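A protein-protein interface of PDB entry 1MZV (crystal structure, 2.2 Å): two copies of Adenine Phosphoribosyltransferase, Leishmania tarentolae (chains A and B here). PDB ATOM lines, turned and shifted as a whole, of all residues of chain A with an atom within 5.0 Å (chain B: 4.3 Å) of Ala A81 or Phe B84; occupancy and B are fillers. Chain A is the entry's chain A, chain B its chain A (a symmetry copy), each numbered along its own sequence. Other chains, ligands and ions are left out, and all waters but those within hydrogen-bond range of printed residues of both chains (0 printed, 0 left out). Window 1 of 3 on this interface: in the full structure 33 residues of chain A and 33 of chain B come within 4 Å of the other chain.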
ATOM      1  N   PHE A  79      28.558 -38.439 -22.742  1.00  0.00           N
ATOM      2  CA  PHE A  79      29.898 -38.094 -22.261  1.00  0.00           C
ATOM      3  C   PHE A  79      29.978 -36.623 -21.812  1.00  0.00           C
ATOM      4  O   PHE A  79      29.555 -35.684 -22.516  1.00  0.00           O
ATOM      5  CB  PHE A  79      30.932 -38.350 -23.353  1.00  0.00           C
ATOM      6  CG  PHE A  79      30.936 -39.783 -23.915  1.00  0.00           C
ATOM      7  CD1 PHE A  79      30.218 -40.835 -23.303  1.00  0.00           C
ATOM      8  CD2 PHE A  79      31.707 -40.077 -25.045  1.00  0.00           C
ATOM      9  CE1 PHE A  79      30.263 -42.126 -23.824  1.00  0.00           C
ATOM     10  CE2 PHE A  79      31.765 -41.370 -25.570  1.00  0.00           C
ATOM     11  CZ  PHE A  79      31.051 -42.392 -24.965  1.00  0.00           C
ATOM     12  N   ASP A  80      30.517 -36.429 -20.625  1.00  0.00           N
ATOM     13  CA  ASP A  80      30.692 -35.112 -20.022  1.00  0.00           C
ATOM     14  C   ASP A  80      31.599 -34.264 -20.919  1.00  0.00           C
ATOM     15  O   ASP A  80      32.660 -34.728 -21.290  1.00  0.00           O
ATOM     16  CB  ASP A  80      31.363 -35.330 -18.672  1.00  0.00           C
ATOM     17  CG  ASP A  80      31.407 -34.091 -17.802  1.00  0.00           C
ATOM     18  OD1 ASP A  80      30.977 -33.009 -18.214  1.00  0.00           O
ATOM     19  OD2 ASP A  80      31.862 -34.128 -16.653  1.00  0.00           O
ATOM     20  N   ALA A  81      31.232 -33.034 -21.294  1.00  0.00           N
ATOM     21  CA  ALA A  81      29.996 -32.350 -20.993  1.00  0.00           C
ATOM     22  C   ALA A  81      29.097 -32.275 -22.227  1.00  0.00           C
ATOM     23  O   ALA A  81      27.917 -31.999 -22.121  1.00  0.00           O
ATOM     24  CB  ALA A  81      30.312 -30.948 -20.556  1.00  0.00           C
ATOM     25  N   ARG A  82      29.652 -32.438 -23.406  1.00  0.00           N
ATOM     26  CA  ARG A  82      28.888 -32.098 -24.591  1.00  0.00           C
ATOM     27  C   ARG A  82      27.902 -33.176 -25.020  1.00  0.00           C
ATOM     28  O   ARG A  82      26.893 -32.895 -25.671  1.00  0.00           O
ATOM     29  CB  ARG A  82      29.836 -31.632 -25.697  1.00  0.00           C
ATOM     30  CG  ARG A  82      30.323 -30.213 -25.414  1.00  0.00           C
ATOM     31  CD  ARG A  82      31.818 -30.090 -25.255  1.00  0.00           C
ATOM     32  NE  ARG A  82      32.331 -30.045 -26.577  1.00  0.00           N
ATOM     33  CZ  ARG A  82      33.573 -30.037 -26.969  1.00  0.00           C
ATOM     34  NH1 ARG A  82      34.614 -30.037 -26.150  1.00  0.00           N
ATOM     35  NH2 ARG A  82      33.747 -30.030 -28.270  1.00  0.00           N
ATOM     36  N   GLY A  83      28.149 -34.401 -24.592  1.00  0.00           N
ATOM     37  CA  GLY A  83      27.169 -35.450 -24.711  1.00  0.00           C
ATOM     38  C   GLY A  83      25.925 -35.180 -23.904  1.00  0.00           C
ATOM     39  O   GLY A  83      24.837 -35.661 -24.251  1.00  0.00           O
ATOM     40  N   PHE A  84      26.078 -34.407 -22.842  1.00  0.00           N
ATOM     41  CA  PHE A  84      24.952 -34.050 -22.008  1.00  0.00           C
ATOM     42  C   PHE A  84      23.947 -33.201 -22.784  1.00  0.00           C
ATOM     43  O   PHE A  84      22.790 -33.142 -22.401  1.00  0.00           O
ATOM     44  CB  PHE A  84      25.354 -33.272 -20.748  1.00  0.00           C
ATOM     45  CG  PHE A  84      26.235 -34.034 -19.781  1.00  0.00           C
ATOM     46  CD1 PHE A  84      26.559 -35.383 -19.965  1.00  0.00           C
ATOM     47  CD2 PHE A  84      26.742 -33.379 -18.679  1.00  0.00           C
ATOM     48  CE1 PHE A  84      27.372 -36.043 -19.052  1.00  0.00           C
ATOM     49  CE2 PHE A  84      27.526 -34.037 -17.761  1.00  0.00           C
ATOM     50  CZ  PHE A  84      27.871 -35.371 -17.972  1.00  0.00           C
ATOM     51  N   LEU A  85      24.401 -32.546 -23.852  1.00  0.00           N
ATOM     52  CA  LEU A  85      23.568 -31.612 -24.573  1.00  0.00           C
ATOM     53  C   LEU A  85      22.569 -32.344 -25.467  1.00  0.00           C
ATOM     54  O   LEU A  85      21.545 -31.781 -25.854  1.00  0.00           O
ATOM     55  CB  LEU A  85      24.445 -30.677 -25.405  1.00  0.00           C
ATOM     56  CG  LEU A  85      25.344 -29.715 -24.654  1.00  0.00           C
ATOM     57  CD1 LEU A  85      26.410 -29.208 -25.565  1.00  0.00           C
ATOM     58  CD2 LEU A  85      24.534 -28.527 -24.028  1.00  0.00           C
ATOM     59  N   GLY B  78      22.046 -22.316 -20.254  1.00  0.00           N
ATOM     60  CA  GLY B  78      22.280 -23.359 -19.275  1.00  0.00           C
ATOM     61  C   GLY B  78      23.712 -23.363 -18.788  1.00  0.00           C
ATOM     62  O   GLY B  78      24.625 -23.071 -19.558  1.00  0.00           O
ATOM     63  N   PHE B  79      23.898 -23.729 -17.518  1.00  0.00           N
ATOM     64  CA  PHE B  79      25.190 -23.655 -16.831  1.00  0.00           C
ATOM     65  C   PHE B  79      25.950 -24.992 -16.908  1.00  0.00           C
ATOM     66  O   PHE B  79      25.414 -26.084 -16.629  1.00  0.00           O
ATOM     67  CB  PHE B  79      24.988 -23.267 -15.370  1.00  0.00           C
ATOM     68  CG  PHE B  79      24.209 -21.957 -15.152  1.00  0.00           C
ATOM     69  CD1 PHE B  79      23.923 -21.064 -16.210  1.00  0.00           C
ATOM     70  CD2 PHE B  79      23.803 -21.605 -13.860  1.00  0.00           C
ATOM     71  CE1 PHE B  79      23.237 -19.875 -15.973  1.00  0.00           C
ATOM     72  CE2 PHE B  79      23.121 -20.411 -13.612  1.00  0.00           C
ATOM     73  CZ  PHE B  79      22.840 -19.547 -14.658  1.00  0.00           C
ATOM     74  N   ASP B  80      27.206 -24.901 -17.298  1.00  0.00           N
ATOM     75  CA  ASP B  80      28.098 -26.048 -17.427  1.00  0.00           C
ATOM     76  C   ASP B  80      28.244 -26.728 -16.063  1.00  0.00           C
ATOM     77  O   ASP B  80      28.529 -26.050 -15.095  1.00  0.00           O
ATOM     78  CB  ASP B  80      29.448 -25.508 -17.880  1.00  0.00           C
ATOM     79  CG  ASP B  80      30.431 -26.584 -18.294  1.00  0.00           C
ATOM     80  OD1 ASP B  80      30.140 -27.781 -18.202  1.00  0.00           O
ATOM     81  OD2 ASP B  80      31.546 -26.297 -18.746  1.00  0.00           O
ATOM     82  N   ALA B  81      28.059 -28.046 -15.933  1.00  0.00           N
ATOM     83  CA  ALA B  81      27.669 -28.989 -16.955  1.00  0.00           C
ATOM     84  C   ALA B  81      26.220 -29.437 -16.764  1.00  0.00           C
ATOM     85  O   ALA B  81      25.618 -29.997 -17.661  1.00  0.00           O
ATOM     86  CB  ALA B  81      28.552 -30.200 -16.860  1.00  0.00           C
ATOM     87  N   ARG B  82      25.674 -29.273 -15.581  1.00  0.00           N
ATOM     88  CA  ARG B  82      24.417 -29.935 -15.293  1.00  0.00           C
ATOM     89  C   ARG B  82      23.196 -29.208 -15.843  1.00  0.00           C
ATOM     90  O   ARG B  82      22.155 -29.814 -16.102  1.00  0.00           O
ATOM     91  CB  ARG B  82      24.337 -30.263 -13.802  1.00  0.00           C
ATOM     92  CG  ARG B  82      25.222 -31.463 -13.476  1.00  0.00           C
ATOM     93  CD  ARG B  82      26.320 -31.174 -12.483  1.00  0.00           C
ATOM     94  NE  ARG B  82      25.699 -31.236 -11.209  1.00  0.00           N
ATOM     95  CZ  ARG B  82      26.206 -30.966 -10.041  1.00  0.00           C
ATOM     96  NH1 ARG B  82      27.463 -30.600  -9.840  1.00  0.00           N
ATOM     97  NH2 ARG B  82      25.372 -31.077  -9.032  1.00  0.00           N
ATOM     98  N   GLY B  83      23.345 -27.920 -16.095  1.00  0.00           N
ATOM     99  CA  GLY B  83      22.363 -27.183 -16.848  1.00  0.00           C
ATOM    100  C   GLY B  83      22.228 -27.673 -18.267  1.00  0.00           C
ATOM    101  O   GLY B  83      21.158 -27.534 -18.878  1.00  0.00           O
ATOM    102  N   PHE B  84      23.298 -28.251 -18.786  1.00  0.00           N
ATOM    103  CA  PHE B  84      23.280 -28.789 -20.127  1.00  0.00           C
ATOM    104  C   PHE B  84      22.298 -29.955 -20.234  1.00  0.00           C
ATOM    105  O   PHE B  84      21.856 -30.269 -21.327  1.00  0.00           O
ATOM    106  CB  PHE B  84      24.653 -29.285 -20.600  1.00  0.00           C
ATOM    107  CG  PHE B  84      25.718 -28.213 -20.703  1.00  0.00           C
ATOM    108  CD1 PHE B  84      25.440 -26.857 -20.499  1.00  0.00           C
ATOM    109  CD2 PHE B  84      27.012 -28.582 -21.005  1.00  0.00           C
ATOM    110  CE1 PHE B  84      26.448 -25.907 -20.603  1.00  0.00           C
ATOM    111  CE2 PHE B  84      28.006 -27.641 -21.134  1.00  0.00           C
ATOM    112  CZ  PHE B  84      27.724 -26.297 -20.895  1.00  0.00           C
ATOM    113  N   LEU B  85      21.982 -30.588 -19.105  1.00  0.00           N
ATOM    114  CA  LEU B  85      21.172 -31.784 -19.113  1.00  0.00           C
ATOM    115  C   LEU B  85      19.696 -31.445 -19.318  1.00  0.00           C
ATOM    116  O   LEU B  85      18.910 -32.296 -19.735  1.00  0.00           O
ATOM    117  CB  LEU B  85      21.369 -32.548 -17.805  1.00  0.00           C
ATOM    118  CG  LEU B  85      22.737 -33.149 -17.549  1.00  0.00           C
ATOM    119  CD1 LEU B  85      22.885 -33.463 -16.099  1.00  0.00           C
ATOM    120  CD2 LEU B  85      22.986 -34.426 -18.425  1.00  0.00           C
ATOM    121  N   PHE B  86      19.323 -30.214 -18.975  1.00  0.00           N
ATOM    122  CA  PHE B  86      17.920 -29.833 -18.950  1.00  0.00           C
ATOM    123  C   PHE B  86      17.522 -28.823 -20.011  1.00  0.00           C
ATOM    124  O   PHE B  86      16.407 -28.854 -20.497  1.00  0.00           O
ATOM    125  CB  PHE B  86      17.576 -29.294 -17.563  1.00  0.00           C
ATOM    126  CG  PHE B  86      17.771 -30.297 -16.490  1.00  0.00           C
ATOM    127  CD1 PHE B  86      16.881 -31.355 -16.353  1.00  0.00           C
ATOM    128  CD2 PHE B  86      18.858 -30.228 -15.650  1.00  0.00           C
ATOM    129  CE1 PHE B  86      17.071 -32.316 -15.388  1.00  0.00           C
ATOM    130  CE2 PHE B  86      19.071 -31.209 -14.703  1.00  0.00           C
ATOM    131  CZ  PHE B  86      18.150 -32.247 -14.562  1.00  0.00           C
ATOM    132  N   GLY B  87      18.426 -27.917 -20.345  1.00  0.00           N
ATOM    133  CA  GLY B  87      18.127 -26.820 -21.244  1.00  0.00           C
ATOM    134  C   GLY B  87      17.714 -27.216 -22.656  1.00  0.00           C
ATOM    135  O   GLY B  87      16.674 -26.739 -23.121  1.00  0.00           O
ATOM    136  N   PRO B  88      18.536 -28.007 -23.343  1.00  0.00           N
ATOM    137  CA  PRO B  88      18.260 -28.469 -24.719  1.00  0.00           C
ATOM    138  C   PRO B  88      16.920 -29.121 -24.917  1.00  0.00           C
ATOM    139  O   PRO B  88      16.257 -28.826 -25.905  1.00  0.00           O
ATOM    140  CB  PRO B  88      19.380 -29.482 -24.995  1.00  0.00           C
ATOM    141  CG  PRO B  88      20.526 -28.982 -24.080  1.00  0.00           C
ATOM    142  CD  PRO B  88      19.869 -28.448 -22.870  1.00  0.00           C
ATOM    143  N   PHE B  98      19.664 -22.700 -27.398  1.00  0.00           N
ATOM    144  CA  PHE B  98      20.294 -23.023 -26.133  1.00  0.00           C
ATOM    145  C   PHE B  98      21.726 -22.562 -26.151  1.00  0.00           C
ATOM    146  O   PHE B  98      22.543 -23.009 -26.991  1.00  0.00           O
ATOM    147  CB  PHE B  98      20.235 -24.497 -25.816  1.00  0.00           C
ATOM    148  CG  PHE B  98      20.872 -24.830 -24.514  1.00  0.00           C
ATOM    149  CD1 PHE B  98      20.250 -24.499 -23.324  1.00  0.00           C
ATOM    150  CD2 PHE B  98      22.129 -25.408 -24.466  1.00  0.00           C
ATOM    151  CE1 PHE B  98      20.856 -24.774 -22.126  1.00  0.00           C
ATOM    152  CE2 PHE B  98      22.728 -25.692 -23.238  1.00  0.00           C
ATOM    153  CZ  PHE B  98      22.107 -25.375 -22.095  1.00  0.00           C
ATOM    154  N   LEU B 100      25.383 -21.718 -23.943  1.00  0.00           N
ATOM    155  CA  LEU B 100      26.225 -22.349 -22.934  1.00  0.00           C
ATOM    156  C   LEU B 100      26.984 -21.325 -22.064  1.00  0.00           C
ATOM    157  O   LEU B 100      27.777 -20.533 -22.579  1.00  0.00           O
ATOM    158  CB  LEU B 100      27.297 -23.213 -23.632  1.00  0.00           C
ATOM    159  CG  LEU B 100      26.838 -24.538 -24.252  1.00  0.00           C
ATOM    160  CD1 LEU B 100      25.681 -24.380 -25.146  1.00  0.00           C
ATOM    161  CD2 LEU B 100      27.975 -25.196 -24.982  1.00  0.00           C
ATOM    162  N   ARG B 102      29.979 -21.374 -19.655  1.00  0.00           N
ATOM    163  CA  ARG B 102      31.123 -22.223 -19.325  1.00  0.00           C
ATOM    164  C   ARG B 102      32.335 -21.425 -18.774  1.00  0.00           C
ATOM    165  O   ARG B 102      32.468 -20.227 -19.035  1.00  0.00           O
ATOM    166  CB  ARG B 102      31.598 -22.950 -20.588  1.00  0.00           C
ATOM    167  CG  ARG B 102      30.509 -23.496 -21.493  1.00  0.00           C
ATOM    168  CD  ARG B 102      30.996 -24.590 -22.416  1.00  0.00           C
ATOM    169  NE  ARG B 102      31.341 -25.752 -21.611  1.00  0.00           N
ATOM    170  CZ  ARG B 102      31.841 -26.872 -22.063  1.00  0.00           C
ATOM    171  NH1 ARG B 102      32.048 -27.041 -23.355  1.00  0.00           N
ATOM    172  NH2 ARG B 102      32.125 -27.838 -21.210  1.00  0.00           N
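NE of Arg B102 lies within salt-bridge range of OD2 of Asp B80 (2.9 Å).
O of Phe A84 sits close to O of Phe B84, at 3.2 Å.
Among the printed residues, pairs that only touch across the chains: Asp A80 with Ala B81 (3.95 Å), Ala A81 with Asp B80 (3.9 Å), Ala A81 with Phe B84 (3.7 Å), Ala A81 with Arg B102 (3.7 Å), Arg A82 with Arg B102 (3.6 Å), Phe A84 with Ala B81 (3.7 Å), Phe A84 with Leu B85 (3.5 Å), Leu A85 with Phe B84 (3.5 Å), Leu A85 with Pro B88 (3.3 Å) and Leu A85 with Phe B98 (3.5 Å).
Of the 7 printed residues of chain A, 5 touch a printed residue of chain B. Of the 14 printed residues of chain B, 7 touch a printed residue of chain A. Among the printed residues, 11 pairs touch across the chains. Among the printed residues, no Asp or Glu carboxylate lies within 4 Å of a Lys or Arg side-chain nitrogen of the other chain.
Asp A80 touches Ala B81, and with the chains exchanged Ala A81 touches Asp B80. Ala A81 touches Phe B84, and with the chains exchanged Phe A84 touches Ala B81. Phe A84 touches its own counterpart, Phe B84. Phe A84 touches Leu B85, and with the chains exchanged Leu A85 touches Phe B84. Of the 11 pairs that touch across the chains among the printed residues, 7 have their exchanged pair printed and touching as well.
Ala A81 touches just these residues of chain B: Asp B80, Phe B84 and Arg B102. Of chain A, only Ala A81, Phe A84 and Leu A85 come within 4 Å of Phe B84. Printed residues of chain B within 4 Å of Asp A80: Ala B81 (3.95 Å). Printed residues of chain B within 4 Å of Leu A85: Phe B84 (3.5 Å), Pro B88 (3.3 Å) and Phe B98 (3.5 Å). Of the printed residues of chain A, Phe B98 touches Leu A85. Of the printed residues of chain A, Ala B81 touches Asp A80 (3.95 Å) and Phe A84 (3.7 Å). Of the printed residues of chain B, Phe A84 touches Ala B81 (3.7 Å), Phe B84 (3.2 Å) and Leu B85 (3.5 Å). The nearest residue of chain B that does not touch Ala A81 is Ala B81 (4.2 Å). The nearest printed residue of chain A that does not touch Leu B85 is Leu A85 (5.7 Å).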
